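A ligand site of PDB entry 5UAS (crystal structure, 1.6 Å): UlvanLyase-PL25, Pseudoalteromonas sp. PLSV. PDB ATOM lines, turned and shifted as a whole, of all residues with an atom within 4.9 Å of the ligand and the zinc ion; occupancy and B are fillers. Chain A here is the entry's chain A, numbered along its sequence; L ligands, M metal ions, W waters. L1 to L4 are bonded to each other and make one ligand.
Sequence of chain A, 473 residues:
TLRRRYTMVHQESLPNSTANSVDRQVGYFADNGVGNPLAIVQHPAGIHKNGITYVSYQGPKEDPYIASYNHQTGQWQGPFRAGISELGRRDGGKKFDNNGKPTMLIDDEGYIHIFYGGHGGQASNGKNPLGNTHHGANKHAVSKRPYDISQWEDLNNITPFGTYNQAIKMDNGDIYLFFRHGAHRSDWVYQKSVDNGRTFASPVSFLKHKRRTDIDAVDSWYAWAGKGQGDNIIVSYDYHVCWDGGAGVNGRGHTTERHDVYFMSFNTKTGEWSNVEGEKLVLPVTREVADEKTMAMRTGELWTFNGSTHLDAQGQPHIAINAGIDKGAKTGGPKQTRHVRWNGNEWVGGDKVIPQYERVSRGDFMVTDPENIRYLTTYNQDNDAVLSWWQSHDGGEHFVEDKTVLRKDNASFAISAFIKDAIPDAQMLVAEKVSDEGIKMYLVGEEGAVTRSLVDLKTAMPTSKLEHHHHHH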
ATOM      1  N   ASN A  36      19.988  29.497   5.044  1.00  0.00           N
ATOM      2  CA  ASN A  36      18.924  28.762   4.370  1.00  0.00           C
ATOM      3  C   ASN A  36      17.617  29.329   4.883  1.00  0.00           C
ATOM      4  O   ASN A  36      17.290  29.093   6.046  1.00  0.00           O
ATOM      5  CB  ASN A  36      19.011  27.274   4.706  1.00  0.00           C
ATOM      6  CG  ASN A  36      20.190  26.595   4.058  1.00  0.00           C
ATOM      7  OD1 ASN A  36      20.461  26.801   2.886  1.00  0.00           O
ATOM      8  ND2 ASN A  36      20.885  25.762   4.813  1.00  0.00           N
ATOM      9  N   ALA A  39      13.111  25.473   4.635  1.00  0.00           N
ATOM     10  CA  ALA A  39      13.428  24.049   4.557  1.00  0.00           C
ATOM     11  C   ALA A  39      12.125  23.281   4.687  1.00  0.00           C
ATOM     12  O   ALA A  39      11.130  23.780   5.201  1.00  0.00           O
ATOM     13  CB  ALA A  39      14.433  23.586   5.643  1.00  0.00           C
ATOM     14  N   LYS A  94      29.212  29.094  13.793  1.00  0.00           N
ATOM     15  CA  LYS A  94      28.739  29.179  12.418  1.00  0.00           C
ATOM     16  C   LYS A  94      28.103  30.538  12.158  1.00  0.00           C
ATOM     17  O   LYS A  94      27.424  31.094  13.015  1.00  0.00           O
ATOM     18  CB  LYS A  94      27.741  28.050  12.156  1.00  0.00           C
ATOM     19  CG  LYS A  94      27.489  27.742  10.711  1.00  0.00           C
ATOM     20  CD  LYS A  94      26.851  26.358  10.538  1.00  0.00           C
ATOM     21  CE  LYS A  94      26.504  26.078   9.082  1.00  0.00           C
ATOM     22  NZ  LYS A  94      25.434  26.994   8.543  1.00  0.00           N
ATOM     23  N   ASP A  97      22.961  29.710  11.663  1.00  0.00           N
ATOM     24  CA  ASP A  97      22.580  28.420  12.215  1.00  0.00           C
ATOM     25  C   ASP A  97      21.463  27.777  11.389  1.00  0.00           C
ATOM     26  O   ASP A  97      21.603  26.624  10.948  1.00  0.00           O
ATOM     27  CB  ASP A  97      22.160  28.629  13.669  1.00  0.00           C
ATOM     28  CG  ASP A  97      21.730  27.358  14.324  1.00  0.00           C
ATOM     29  OD1 ASP A  97      20.761  26.753  13.843  1.00  0.00           O
ATOM     30  OD2 ASP A  97      22.347  26.983  15.325  1.00  0.00           O
ATOM     31  N   ASN A  98      20.362  28.510  11.148  1.00  0.00           N
ATOM     32  CA  ASN A  98      19.261  28.160  10.277  1.00  0.00           C
ATOM     33  C   ASN A  98      18.234  27.192  10.884  1.00  0.00           C
ATOM     34  O   ASN A  98      17.145  27.036  10.291  1.00  0.00           O
ATOM     35  CB  ASN A  98      19.716  27.548   8.938  1.00  0.00           C
ATOM     36  CG  ASN A  98      20.678  28.442   8.181  1.00  0.00           C
ATOM     37  OD1 ASN A  98      20.411  29.615   7.945  1.00  0.00           O
ATOM     38  ND2 ASN A  98      21.805  27.853   7.768  1.00  0.00           N
ATOM     39  N   ASN A  99      18.520  26.537  12.001  1.00  0.00           N
ATOM     40  CA  ASN A  99      17.612  25.501  12.489  1.00  0.00           C
ATOM     41  C   ASN A  99      16.398  26.077  13.193  1.00  0.00           C
ATOM     42  O   ASN A  99      15.487  25.320  13.528  1.00  0.00           O
ATOM     43  CB  ASN A  99      18.347  24.540  13.430  1.00  0.00           C
ATOM     44  CG  ASN A  99      19.314  23.638  12.652  1.00  0.00           C
ATOM     45  OD1 ASN A  99      18.926  22.590  12.161  1.00  0.00           O
ATOM     46  ND2 ASN A  99      20.568  24.056  12.540  1.00  0.00           N
ATOM     47  N   LYS A 101      14.547  28.711  11.653  1.00  0.00           N
ATOM     48  CA  LYS A 101      13.672  29.386  10.695  1.00  0.00           C
ATOM     49  C   LYS A 101      12.220  29.048  11.018  1.00  0.00           C
ATOM     50  O   LYS A 101      11.946  28.045  11.693  1.00  0.00           O
ATOM     51  CB  LYS A 101      14.042  28.999   9.255  1.00  0.00           C
ATOM     52  CG  LYS A 101      13.808  27.495   8.930  1.00  0.00           C
ATOM     53  CD  LYS A 101      14.259  27.127   7.462  1.00  0.00           C
ATOM     54  CE  LYS A 101      15.750  26.735   7.344  1.00  0.00           C
ATOM     55  NZ  LYS A 101      16.128  25.570   8.284  1.00  0.00           N
ATOM     56  N   HIS A 119      17.435  25.927  18.579  1.00  0.00           N
ATOM     57  CA  HIS A 119      18.376  24.869  18.216  1.00  0.00           C
ATOM     58  C   HIS A 119      18.790  24.141  19.490  1.00  0.00           C
ATOM     59  O   HIS A 119      19.965  23.848  19.727  1.00  0.00           O
ATOM     60  CB  HIS A 119      19.584  25.428  17.449  1.00  0.00           C
ATOM     61  CG  HIS A 119      20.351  24.369  16.718  1.00  0.00           C
ATOM     62  ND1 HIS A 119      21.457  24.647  15.952  1.00  0.00           N
ATOM     63  CD2 HIS A 119      20.148  23.024  16.616  1.00  0.00           C
ATOM     64  CE1 HIS A 119      21.929  23.532  15.413  1.00  0.00           C
ATOM     65  NE2 HIS A 119      21.138  22.530  15.791  1.00  0.00           N
ATOM     66  N   HIS A 134      22.138  22.865  22.863  1.00  0.00           N
ATOM     67  CA  HIS A 134      23.163  23.419  21.996  1.00  0.00           C
ATOM     68  C   HIS A 134      23.119  24.932  22.169  1.00  0.00           C
ATOM     69  O   HIS A 134      23.771  25.453  23.085  1.00  0.00           O
ATOM     70  CB  HIS A 134      22.958  22.975  20.544  1.00  0.00           C
ATOM     71  CG  HIS A 134      24.050  23.444  19.625  1.00  0.00           C
ATOM     72  ND1 HIS A 134      25.380  23.387  19.947  1.00  0.00           N
ATOM     73  CD2 HIS A 134      23.987  24.005  18.390  1.00  0.00           C
ATOM     74  CE1 HIS A 134      26.108  23.877  18.962  1.00  0.00           C
ATOM     75  NE2 HIS A 134      25.292  24.253  18.004  1.00  0.00           N
ATOM     76  N   TYR A 164      13.245  22.089  15.205  1.00  0.00           N
ATOM     77  CA  TYR A 164      12.422  21.549  14.121  1.00  0.00           C
ATOM     78  C   TYR A 164      10.938  21.563  14.406  1.00  0.00           C
ATOM     79  O   TYR A 164      10.273  20.519  14.408  1.00  0.00           O
ATOM     80  CB  TYR A 164      12.863  20.115  13.748  1.00  0.00           C
ATOM     81  CG  TYR A 164      14.330  20.045  13.390  1.00  0.00           C
ATOM     82  CD1 TYR A 164      14.838  20.815  12.355  1.00  0.00           C
ATOM     83  CD2 TYR A 164      15.222  19.276  14.136  1.00  0.00           C
ATOM     84  CE1 TYR A 164      16.192  20.757  12.008  1.00  0.00           C
ATOM     85  CE2 TYR A 164      16.581  19.228  13.824  1.00  0.00           C
ATOM     86  CZ  TYR A 164      17.059  19.977  12.738  1.00  0.00           C
ATOM     87  OH  TYR A 164      18.397  19.954  12.429  1.00  0.00           O
ATOM     88  N   ARG A 180      12.006  18.201  18.123  1.00  0.00           N
ATOM     89  CA  ARG A 180      13.024  17.496  18.900  1.00  0.00           C
ATOM     90  C   ARG A 180      13.322  18.276  20.178  1.00  0.00           C
ATOM     91  O   ARG A 180      13.628  19.478  20.119  1.00  0.00           O
ATOM     92  CB  ARG A 180      14.267  17.319  18.045  1.00  0.00           C
ATOM     93  CG  ARG A 180      15.363  16.572  18.766  1.00  0.00           C
ATOM     94  CD  ARG A 180      16.602  16.542  17.872  1.00  0.00           C
ATOM     95  NE  ARG A 180      17.189  17.876  17.733  1.00  0.00           N
ATOM     96  CZ  ARG A 180      18.201  18.196  16.939  1.00  0.00           C
ATOM     97  NH1 ARG A 180      18.743  17.271  16.120  1.00  0.00           N
ATOM     98  NH2 ARG A 180      18.654  19.458  16.920  1.00  0.00           N
ATOM     99  N   ALA A 183      19.004  19.117  21.360  1.00  0.00           N
ATOM    100  CA  ALA A 183      19.894  18.951  20.212  1.00  0.00           C
ATOM    101  C   ALA A 183      19.908  17.473  19.804  1.00  0.00           C
ATOM    102  O   ALA A 183      18.894  16.802  19.997  1.00  0.00           O
ATOM    103  CB  ALA A 183      21.289  19.490  20.536  1.00  0.00           C
ATOM    104  N   HIS A 184      21.010  16.952  19.244  1.00  0.00           N
ATOM    105  CA  HIS A 184      20.941  15.611  18.650  1.00  0.00           C
ATOM    106  C   HIS A 184      20.440  14.560  19.633  1.00  0.00           C
ATOM    107  O   HIS A 184      19.721  13.618  19.255  1.00  0.00           O
ATOM    108  CB  HIS A 184      22.309  15.154  18.168  1.00  0.00           C
ATOM    109  CG  HIS A 184      22.764  15.813  16.922  1.00  0.00           C
ATOM    110  ND1 HIS A 184      23.717  15.251  16.104  1.00  0.00           N
ATOM    111  CD2 HIS A 184      22.425  16.996  16.370  1.00  0.00           C
ATOM    112  CE1 HIS A 184      23.923  16.054  15.066  1.00  0.00           C
ATOM    113  NE2 HIS A 184      23.172  17.131  15.220  1.00  0.00           N
ATOM    114  N   TYR A 222      15.299  12.066  13.113  1.00  0.00           N
ATOM    115  CA  TYR A 222      14.729  13.245  12.463  1.00  0.00           C
ATOM    116  C   TYR A 222      13.358  12.842  11.917  1.00  0.00           C
ATOM    117  O   TYR A 222      13.273  11.945  11.093  1.00  0.00           O
ATOM    118  CB  TYR A 222      15.652  13.780  11.345  1.00  0.00           C
ATOM    119  CG  TYR A 222      16.973  14.309  11.845  1.00  0.00           C
ATOM    120  CD1 TYR A 222      18.083  13.492  11.937  1.00  0.00           C
ATOM    121  CD2 TYR A 222      17.133  15.652  12.191  1.00  0.00           C
ATOM    122  CE1 TYR A 222      19.312  13.984  12.394  1.00  0.00           C
ATOM    123  CE2 TYR A 222      18.362  16.144  12.647  1.00  0.00           C
ATOM    124  CZ  TYR A 222      19.436  15.301  12.752  1.00  0.00           C
ATOM    125  OH  TYR A 222      20.672  15.751  13.210  1.00  0.00           O
ATOM    126  N   HIS A 240      19.519   8.717  12.974  1.00  0.00           N
ATOM    127  CA  HIS A 240      20.842   9.325  13.027  1.00  0.00           C
ATOM    128  C   HIS A 240      21.711   8.484  13.952  1.00  0.00           C
ATOM    129  O   HIS A 240      21.403   8.309  15.140  1.00  0.00           O
ATOM    130  CB  HIS A 240      20.740  10.772  13.514  1.00  0.00           C
ATOM    131  CG  HIS A 240      22.055  11.415  13.870  1.00  0.00           C
ATOM    132  ND1 HIS A 240      23.161  11.355  13.042  1.00  0.00           N
ATOM    133  CD2 HIS A 240      22.421  12.159  14.943  1.00  0.00           C
ATOM    134  CE1 HIS A 240      24.158  12.011  13.614  1.00  0.00           C
ATOM    135  NE2 HIS A 240      23.737  12.512  14.767  1.00  0.00           N
ATOM    136  N   CYS A 242      24.430   8.714  16.084  1.00  0.00           N
ATOM    137  CA  CYS A 242      25.085   9.859  16.716  1.00  0.00           C
ATOM    138  C   CYS A 242      26.339   9.372  17.428  1.00  0.00           C
ATOM    139  O   CYS A 242      26.334   9.028  18.618  1.00  0.00           O
ATOM    140  CB  CYS A 242      24.125  10.577  17.652  1.00  0.00           C
ATOM    141  SG  CYS A 242      24.700  12.245  18.118  1.00  0.00           S
ATOM    142  N   HIS A 254      32.019  12.191  15.114  1.00  0.00           N
ATOM    143  CA  HIS A 254      30.613  12.539  14.955  1.00  0.00           C
ATOM    144  C   HIS A 254      30.394  13.221  13.608  1.00  0.00           C
ATOM    145  O   HIS A 254      31.012  14.251  13.312  1.00  0.00           O
ATOM    146  CB  HIS A 254      30.151  13.428  16.116  1.00  0.00           C
ATOM    147  CG  HIS A 254      28.731  13.868  15.980  1.00  0.00           C
ATOM    148  ND1 HIS A 254      28.377  15.053  15.385  1.00  0.00           N
ATOM    149  CD2 HIS A 254      27.569  13.260  16.323  1.00  0.00           C
ATOM    150  CE1 HIS A 254      27.059  15.172  15.397  1.00  0.00           C
ATOM    151  NE2 HIS A 254      26.545  14.099  15.969  1.00  0.00           N
ATOM    152  N   THR A 255      29.516  12.651  12.814  1.00  0.00           N
ATOM    153  CA  THR A 255      29.133  13.145  11.498  1.00  0.00           C
ATOM    154  C   THR A 255      27.623  13.378  11.494  1.00  0.00           C
ATOM    155  O   THR A 255      26.958  13.286  12.538  1.00  0.00           O
ATOM    156  CB  THR A 255      29.495  12.124  10.435  1.00  0.00           C
ATOM    157  OG1 THR A 255      28.760  10.926  10.710  1.00  0.00           O
ATOM    158  CG2 THR A 255      30.998  11.814  10.475  1.00  0.00           C
ATOM    159  N   THR A 256      27.064  13.659  10.311  1.00  0.00           N
ATOM    160  CA  THR A 256      25.615  13.692  10.128  1.00  0.00           C
ATOM    161  C   THR A 256      25.060  12.340   9.652  1.00  0.00           C
ATOM    162  O   THR A 256      23.949  12.305   9.100  1.00  0.00           O
ATOM    163  CB  THR A 256      25.196  14.791   9.143  1.00  0.00           C
ATOM    164  OG1 THR A 256      25.682  14.499   7.825  1.00  0.00           O
ATOM    165  CG2 THR A 256      25.730  16.160   9.609  1.00  0.00           C
ATOM    166  N   ARG A 258      23.071   9.414   8.723  1.00  0.00           N
ATOM    167  CA  ARG A 258      21.688   9.024   8.930  1.00  0.00           C
ATOM    168  C   ARG A 258      21.370   7.886   7.973  1.00  0.00           C
ATOM    169  O   ARG A 258      21.961   7.793   6.897  1.00  0.00           O
ATOM    170  CB  ARG A 258      20.736  10.216   8.691  1.00  0.00           C
ATOM    171  CG  ARG A 258      20.948  11.391   9.676  1.00  0.00           C
ATOM    172  CD  ARG A 258      20.533  12.745   9.066  1.00  0.00           C
ATOM    173  NE  ARG A 258      19.103  12.832   8.768  1.00  0.00           N
ATOM    174  CZ  ARG A 258      18.400  13.961   8.677  1.00  0.00           C
ATOM    175  NH1 ARG A 258      18.993  15.147   8.877  1.00  0.00           N
ATOM    176  NH2 ARG A 258      17.084  13.894   8.396  1.00  0.00           N
ATOM    177  N   PHE A 305      18.652  12.035   4.198  1.00  0.00           N
ATOM    178  CA  PHE A 305      18.197  13.316   4.701  1.00  0.00           C
ATOM    179  C   PHE A 305      16.690  13.297   4.516  1.00  0.00           C
ATOM    180  O   PHE A 305      16.216  13.065   3.406  1.00  0.00           O
ATOM    181  CB  PHE A 305      18.851  14.500   3.939  1.00  0.00           C
ATOM    182  CG  PHE A 305      18.485  15.832   4.485  1.00  0.00           C
ATOM    183  CD1 PHE A 305      19.148  16.328   5.596  1.00  0.00           C
ATOM    184  CD2 PHE A 305      17.505  16.608   3.871  1.00  0.00           C
ATOM    185  CE1 PHE A 305      18.809  17.536   6.155  1.00  0.00           C
ATOM    186  CE2 PHE A 305      17.165  17.857   4.394  1.00  0.00           C
ATOM    187  CZ  PHE A 305      17.853  18.329   5.527  1.00  0.00           C
ATOM    188  N   LYS A 330      31.860  15.267   6.105  1.00  0.00           N
ATOM    189  CA  LYS A 330      31.149  15.280   7.374  1.00  0.00           C
ATOM    190  C   LYS A 330      29.648  15.074   7.177  1.00  0.00           C
ATOM    191  O   LYS A 330      28.967  14.536   8.054  1.00  0.00           O
ATOM    192  CB  LYS A 330      31.411  16.599   8.095  1.00  0.00           C
ATOM    193  CG  LYS A 330      30.626  16.745   9.384  1.00  0.00           C
ATOM    194  CD  LYS A 330      31.339  16.098  10.542  1.00  0.00           C
ATOM    195  CE  LYS A 330      32.426  17.010  11.087  1.00  0.00           C
ATOM    196  NZ  LYS A 330      31.855  18.320  11.530  1.00  0.00           N
ATOM    197  N   THR A 331      29.124  15.477   6.021  1.00  0.00           N
ATOM    198  CA  THR A 331      27.737  15.217   5.662  1.00  0.00           C
ATOM    199  C   THR A 331      27.603  14.047   4.684  1.00  0.00           C
ATOM    200  O   THR A 331      26.555  13.868   4.069  1.00  0.00           O
ATOM    201  CB  THR A 331      27.098  16.465   5.040  1.00  0.00           C
ATOM    202  OG1 THR A 331      27.950  16.950   3.988  1.00  0.00           O
ATOM    203  CG2 THR A 331      26.930  17.565   6.093  1.00  0.00           C
ATOM    204  N   ARG A 362      15.944  18.037  -3.775  1.00  0.00           N
ATOM    205  CA  ARG A 362      14.963  18.044  -2.691  1.00  0.00           C
ATOM    206  C   ARG A 362      13.619  18.299  -3.325  1.00  0.00           C
ATOM    207  O   ARG A 362      13.546  18.917  -4.376  1.00  0.00           O
ATOM    208  CB  ARG A 362      15.238  19.165  -1.659  1.00  0.00           C
ATOM    209  CG  ARG A 362      16.583  19.078  -0.960  1.00  0.00           C
ATOM    210  CD  ARG A 362      16.612  17.862   0.010  1.00  0.00           C
ATOM    211  NE  ARG A 362      17.869  17.842   0.741  1.00  0.00           N
ATOM    212  CZ  ARG A 362      18.946  17.121   0.404  1.00  0.00           C
ATOM    213  NH1 ARG A 362      18.910  16.319  -0.660  1.00  0.00           N
ATOM    214  NH2 ARG A 362      20.056  17.214   1.131  1.00  0.00           N
ATOM    215  N   LYS A 433      19.349  31.240  -3.117  1.00  0.00           N
ATOM    216  CA  LYS A 433      20.643  31.352  -2.436  1.00  0.00           C
ATOM    217  C   LYS A 433      21.723  31.737  -3.425  1.00  0.00           C
ATOM    218  O   LYS A 433      22.024  30.993  -4.353  1.00  0.00           O
ATOM    219  CB  LYS A 433      21.000  30.021  -1.743  1.00  0.00           C
ATOM    220  CG  LYS A 433      19.936  29.654  -0.717  1.00  0.00           C
ATOM    221  CD  LYS A 433      20.093  28.279  -0.043  1.00  0.00           C
ATOM    222  CE  LYS A 433      21.336  27.546  -0.388  1.00  0.00           C
ATOM    223  NZ  LYS A 433      21.252  26.182   0.239  1.00  0.00           N
HETATM  224  C1  LIG L   1      26.792  19.649  17.782  1.00  0.00           C
HETATM  225  C2  LIG L   1      27.362  19.889  16.390  1.00  0.00           C
HETATM  226  C3  LIG L   1      26.372  19.460  15.322  1.00  0.00           C
HETATM  227  C4  LIG L   1      25.062  20.239  15.496  1.00  0.00           C
HETATM  228  C5  LIG L   1      24.556  19.917  16.912  1.00  0.00           C
HETATM  229  C6  LIG L   1      23.253  20.612  17.253  1.00  0.00           C
HETATM  230  O1  LIG L   1      26.645  18.235  17.996  1.00  0.00           O
HETATM  231  O2  LIG L   1      27.631  18.735  11.825  1.00  0.00           O
HETATM  232  O3  LIG L   1      27.682  21.274  16.223  1.00  0.00           O
HETATM  233  O4  LIG L   1      28.390  17.599  13.822  1.00  0.00           O
HETATM  234  O5  LIG L   1      26.936  19.610  14.025  1.00  0.00           O
HETATM  235  O6  LIG L   1      26.083  17.444  13.150  1.00  0.00           O
HETATM  236  O7  LIG L   1      25.523  20.310  17.895  1.00  0.00           O
HETATM  237  S1  LIG L   1      27.268  18.332  13.214  1.00  0.00           S
HETATM  238  O8  LIG L   1      24.112  19.827  14.499  1.00  0.00           O
HETATM  239  C1  LG2 L   2      23.868  20.770  13.441  1.00  0.00           C
HETATM  240  C2  LG2 L   2      24.273  20.156  12.083  1.00  0.00           C
HETATM  241  C3  LG2 L   2      23.298  19.060  11.806  1.00  0.00           C
HETATM  242  C4  LG2 L   2      21.885  19.543  11.812  1.00  0.00           C
HETATM  243  C5  LG2 L   2      21.577  20.211  13.091  1.00  0.00           C
HETATM  244  C6  LG2 L   2      21.008  19.345  14.264  1.00  0.00           C
HETATM  245  O1  LG2 L   2      24.259  21.179  11.078  1.00  0.00           O
HETATM  246  O2  LG2 L   2      23.505  17.899  12.629  1.00  0.00           O
HETATM  247  O3  LG2 L   2      21.368  20.270  10.684  1.00  0.00           O
HETATM  248  O4  LG2 L   2      22.469  21.194  13.503  1.00  0.00           O
HETATM  249  O5  LG2 L   2      20.522  18.232  14.057  1.00  0.00           O
HETATM  250  O6  LG2 L   2      21.025  19.804  15.415  1.00  0.00           O
HETATM  251  C1  LG3 L   3      20.511  19.597   9.761  1.00  0.00           C
HETATM  252  C2  LG3 L   3      19.735  20.700   9.062  1.00  0.00           C
HETATM  253  C3  LG3 L   3      20.674  21.617   8.266  1.00  0.00           C
HETATM  254  C4  LG3 L   3      21.613  20.846   7.333  1.00  0.00           C
HETATM  255  C5  LG3 L   3      22.263  19.706   8.095  1.00  0.00           C
HETATM  256  C6  LG3 L   3      23.027  18.807   7.119  1.00  0.00           C
HETATM  257  O1  LG3 L   3      18.614  24.553   7.105  1.00  0.00           O
HETATM  258  O2  LG3 L   3      18.777  20.114   8.208  1.00  0.00           O
HETATM  259  O3  LG3 L   3      21.049  24.650   7.659  1.00  0.00           O
HETATM  260  O4  LG3 L   3      19.872  22.514   7.520  1.00  0.00           O
HETATM  261  O5  LG3 L   3      19.377  24.094   9.321  1.00  0.00           O
HETATM  262  O6  LG3 L   3      21.330  18.915   8.831  1.00  0.00           O
HETATM  263  S1  LG3 L   3      19.736  24.022   7.901  1.00  0.00           S
HETATM  264  O7  LG3 L   3      22.676  21.698   6.869  1.00  0.00           O
HETATM  265  C1  LG4 L   4      22.434  22.200   5.553  1.00  0.00           C
HETATM  266  C2  LG4 L   4      23.361  23.393   5.316  1.00  0.00           C
HETATM  267  C3  LG4 L   4      24.801  22.938   5.519  1.00  0.00           C
HETATM  268  C4  LG4 L   4      25.069  21.661   4.774  1.00  0.00           C
HETATM  269  C5  LG4 L   4      24.079  20.856   4.353  1.00  0.00           C
HETATM  270  C6  LG4 L   4      24.396  19.656   3.585  1.00  0.00           C
HETATM  271  O1  LG4 L   4      23.161  23.922   3.994  1.00  0.00           O
HETATM  272  O2  LG4 L   4      25.114  22.722   6.893  1.00  0.00           O
HETATM  273  O3  LG4 L   4      22.688  21.168   4.601  1.00  0.00           O
HETATM  274  O4  LG4 L   4      25.592  19.426   3.274  1.00  0.00           O
HETATM  275  O5  LG4 L   4      23.477  18.900   3.228  1.00  0.00           O
HETATM  276 ZN    ZN M   1      24.738  13.479  16.275  1.00  0.00          ZN
HETATM  277  O   HOH W   1      22.472  16.097   4.163  1.00  0.00           O
HETATM  278  O   HOH W   2      22.890  15.423  11.420  1.00  0.00           O
HETATM  279  O   HOH W   3      23.723  25.320   9.106  1.00  0.00           O
HETATM  280  O   HOH W   4      17.819  22.865   5.004  1.00  0.00           O
HETATM  281  O   HOH W   5      19.587  21.223   3.926  1.00  0.00           O
HETATM  282  O   HOH W   6      16.749  23.041   9.565  1.00  0.00           O
HETATM  283  O   HOH W   7      17.520  17.829   9.681  1.00  0.00           O
HETATM  284  O   HOH W   8      25.043  24.269   2.249  1.00  0.00           O
HETATM  285  O   HOH W   9      21.139  22.936   2.428  1.00  0.00           O
HETATM  286  O   HOH W  10      21.664  15.992   9.060  1.00  0.00           O
HETATM  287  O   HOH W  11      23.163  19.279   0.333  1.00  0.00           O
HETATM  288  O   HOH W  12      20.879  18.730   3.438  1.00  0.00           O
HETATM  289  O   HOH W  13      26.630  15.746  20.007  1.00  0.00           O
HETATM  290  O   HOH W  14      23.754  17.526  19.681  1.00  0.00           O
HETATM  291  O   HOH W  15      16.641  21.479   7.207  1.00  0.00           O
HETATM  292  O   HOH W  16      22.808  23.429  10.872  1.00  0.00           O
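The zinc ion is bound by NE2 of His 254 (1.9 Å), NE2 of His 240 (2.1 Å), ND1 of His 184 (2.1 Å) and SG of Cys 242 (2.2 Å). The zinc ion has four donor atoms within binding distance.
Residues that only touch the ligand: Asp 97 (3.7 Å), His 134 (3.7 Å), Ala 183 (3.99 Å), Thr 256 (3.8 Å) and Phe 305 (3.3 Å). Hydrophobic or aromatic side chains that line the ligand: His 119, His 134, Ala 183, His 184, Tyr 222, His 254 and Phe 305. 16 residues have an atom within 4 Å of the ligand: Asn 36, Asp 97, Asn 98, Asn 99, Lys 101, His 119, His 134, Tyr 164, Arg 180, Ala 183, His 184, Tyr 222, His 254, Thr 256, Phe 305 and Thr 331. The nearest printed residue that does not touch the ligand is Lys 330 (4.2 Å).
A ring nitrogen (NE2) of His 184 lies within hydrogen-bond range of the side-chain hydroxyl of Tyr 222. ND1 of His 119 sits at hydrogen-bond distance from OD2 of Asp 97 (2.6 Å). NE of Arg 180 lies within hydrogen-bond range of O of Ala 183, at 3.0 Å. The backbone carbonyl oxygen (O) of Asn 98 lies within hydrogen-bond range of the side-chain amino group (NZ) of Lys 101 (2.7 Å). The side-chain amide oxygen (OD1) of Asn 98 sits at hydrogen-bond distance from the backbone NH (N) of Asn 36 (2.9 Å). NZ of Lys 433 lies within hydrogen-bond range of OD1 of Asn 36 (2.8 Å). The side-chain amide oxygen of Asn 99 lies within hydrogen-bond range of the side-chain hydroxyl of Tyr 164, at 2.7 Å. The backbone carbonyl oxygen of Lys 330 lies within hydrogen-bond range of the backbone NH of Thr 256.
Four residues have an atom within 4 Å of the zinc ion: His 184, His 240, Cys 242 and His 254. The nearest printed residue that does not touch the zinc ion is Thr 255 (4.4 Å).
O4 of LIG L1 sits at hydrogen-bond distance from ND1 of His 254 (3.0 Å). A ring nitrogen (NE2) of His 184 sits at hydrogen-bond distance from an oxygen (O2) of LG2 L2. The side-chain hydroxyl (OH) of Tyr 222 sits at hydrogen-bond distance from an oxygen (O5) of LG2 L2 (2.6 Å). An oxygen (O6) of LG2 L2 sits at hydrogen-bond distance from a ring nitrogen (NE2) of His 119 (2.8 Å). NH2 of Arg 180 lies within salt-bridge range of O6 of LG2 L2 (2.8 Å). The side-chain amino group (NZ) of Lys 101 is in salt-bridge range of an oxygen (O1) of LG3 L3 (2.9 Å). An oxygen (O1) of LG4 L4 lies within hydrogen-bond range of the side-chain amide nitrogen (ND2) of Asn 36 (3.0 Å). An oxygen (O5) of LG2 L2 sits at hydrogen-bond distance from the side-chain hydroxyl of Tyr 164 (3.2 Å). OD1 of Asn 99 sits close to O5 of LG3 L3. An oxygen (O3) of LG3 L3 sits at hydrogen-bond distance from the side-chain amide nitrogen (ND2) of Asn 98 (3.3 Å). The side-chain hydroxyl of Thr 331 lies within hydrogen-bond range of an oxygen (O4) of LG4 L4 (3.5 Å).
Water W16 lies within hydrogen-bond range of O1 of LG2 L2 (2.7 Å), ND2 of Asn 99 (2.9 Å) and O of Asp 97 (3.4 Å). Water W2 lies within hydrogen-bond range of O2 of LG2 L2 and OH of Tyr 222. Water W10 lies within hydrogen-bond range of NH1 of Arg 258 (2.8 Å) and O6 of LG3 L3 (3.0 Å). Water W7 lies within hydrogen-bond range of O2 of LG3 L3 (3.0 Å) and NH1 of Arg 258 (3.2 Å). Water W3 lies within hydrogen-bond range of the side-chain amino group of Lys 94 (2.5 Å), the backbone carbonyl oxygen of Asp 97 (3.1 Å), an oxygen (O3) of LG3 L3 (3.1 Å) and the side-chain amide nitrogen of Asn 98 (3.4 Å). Water W14 lies within hydrogen-bond range of N of His 184 (2.8 Å) and O1 of LIG L1 (3.4 Å).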
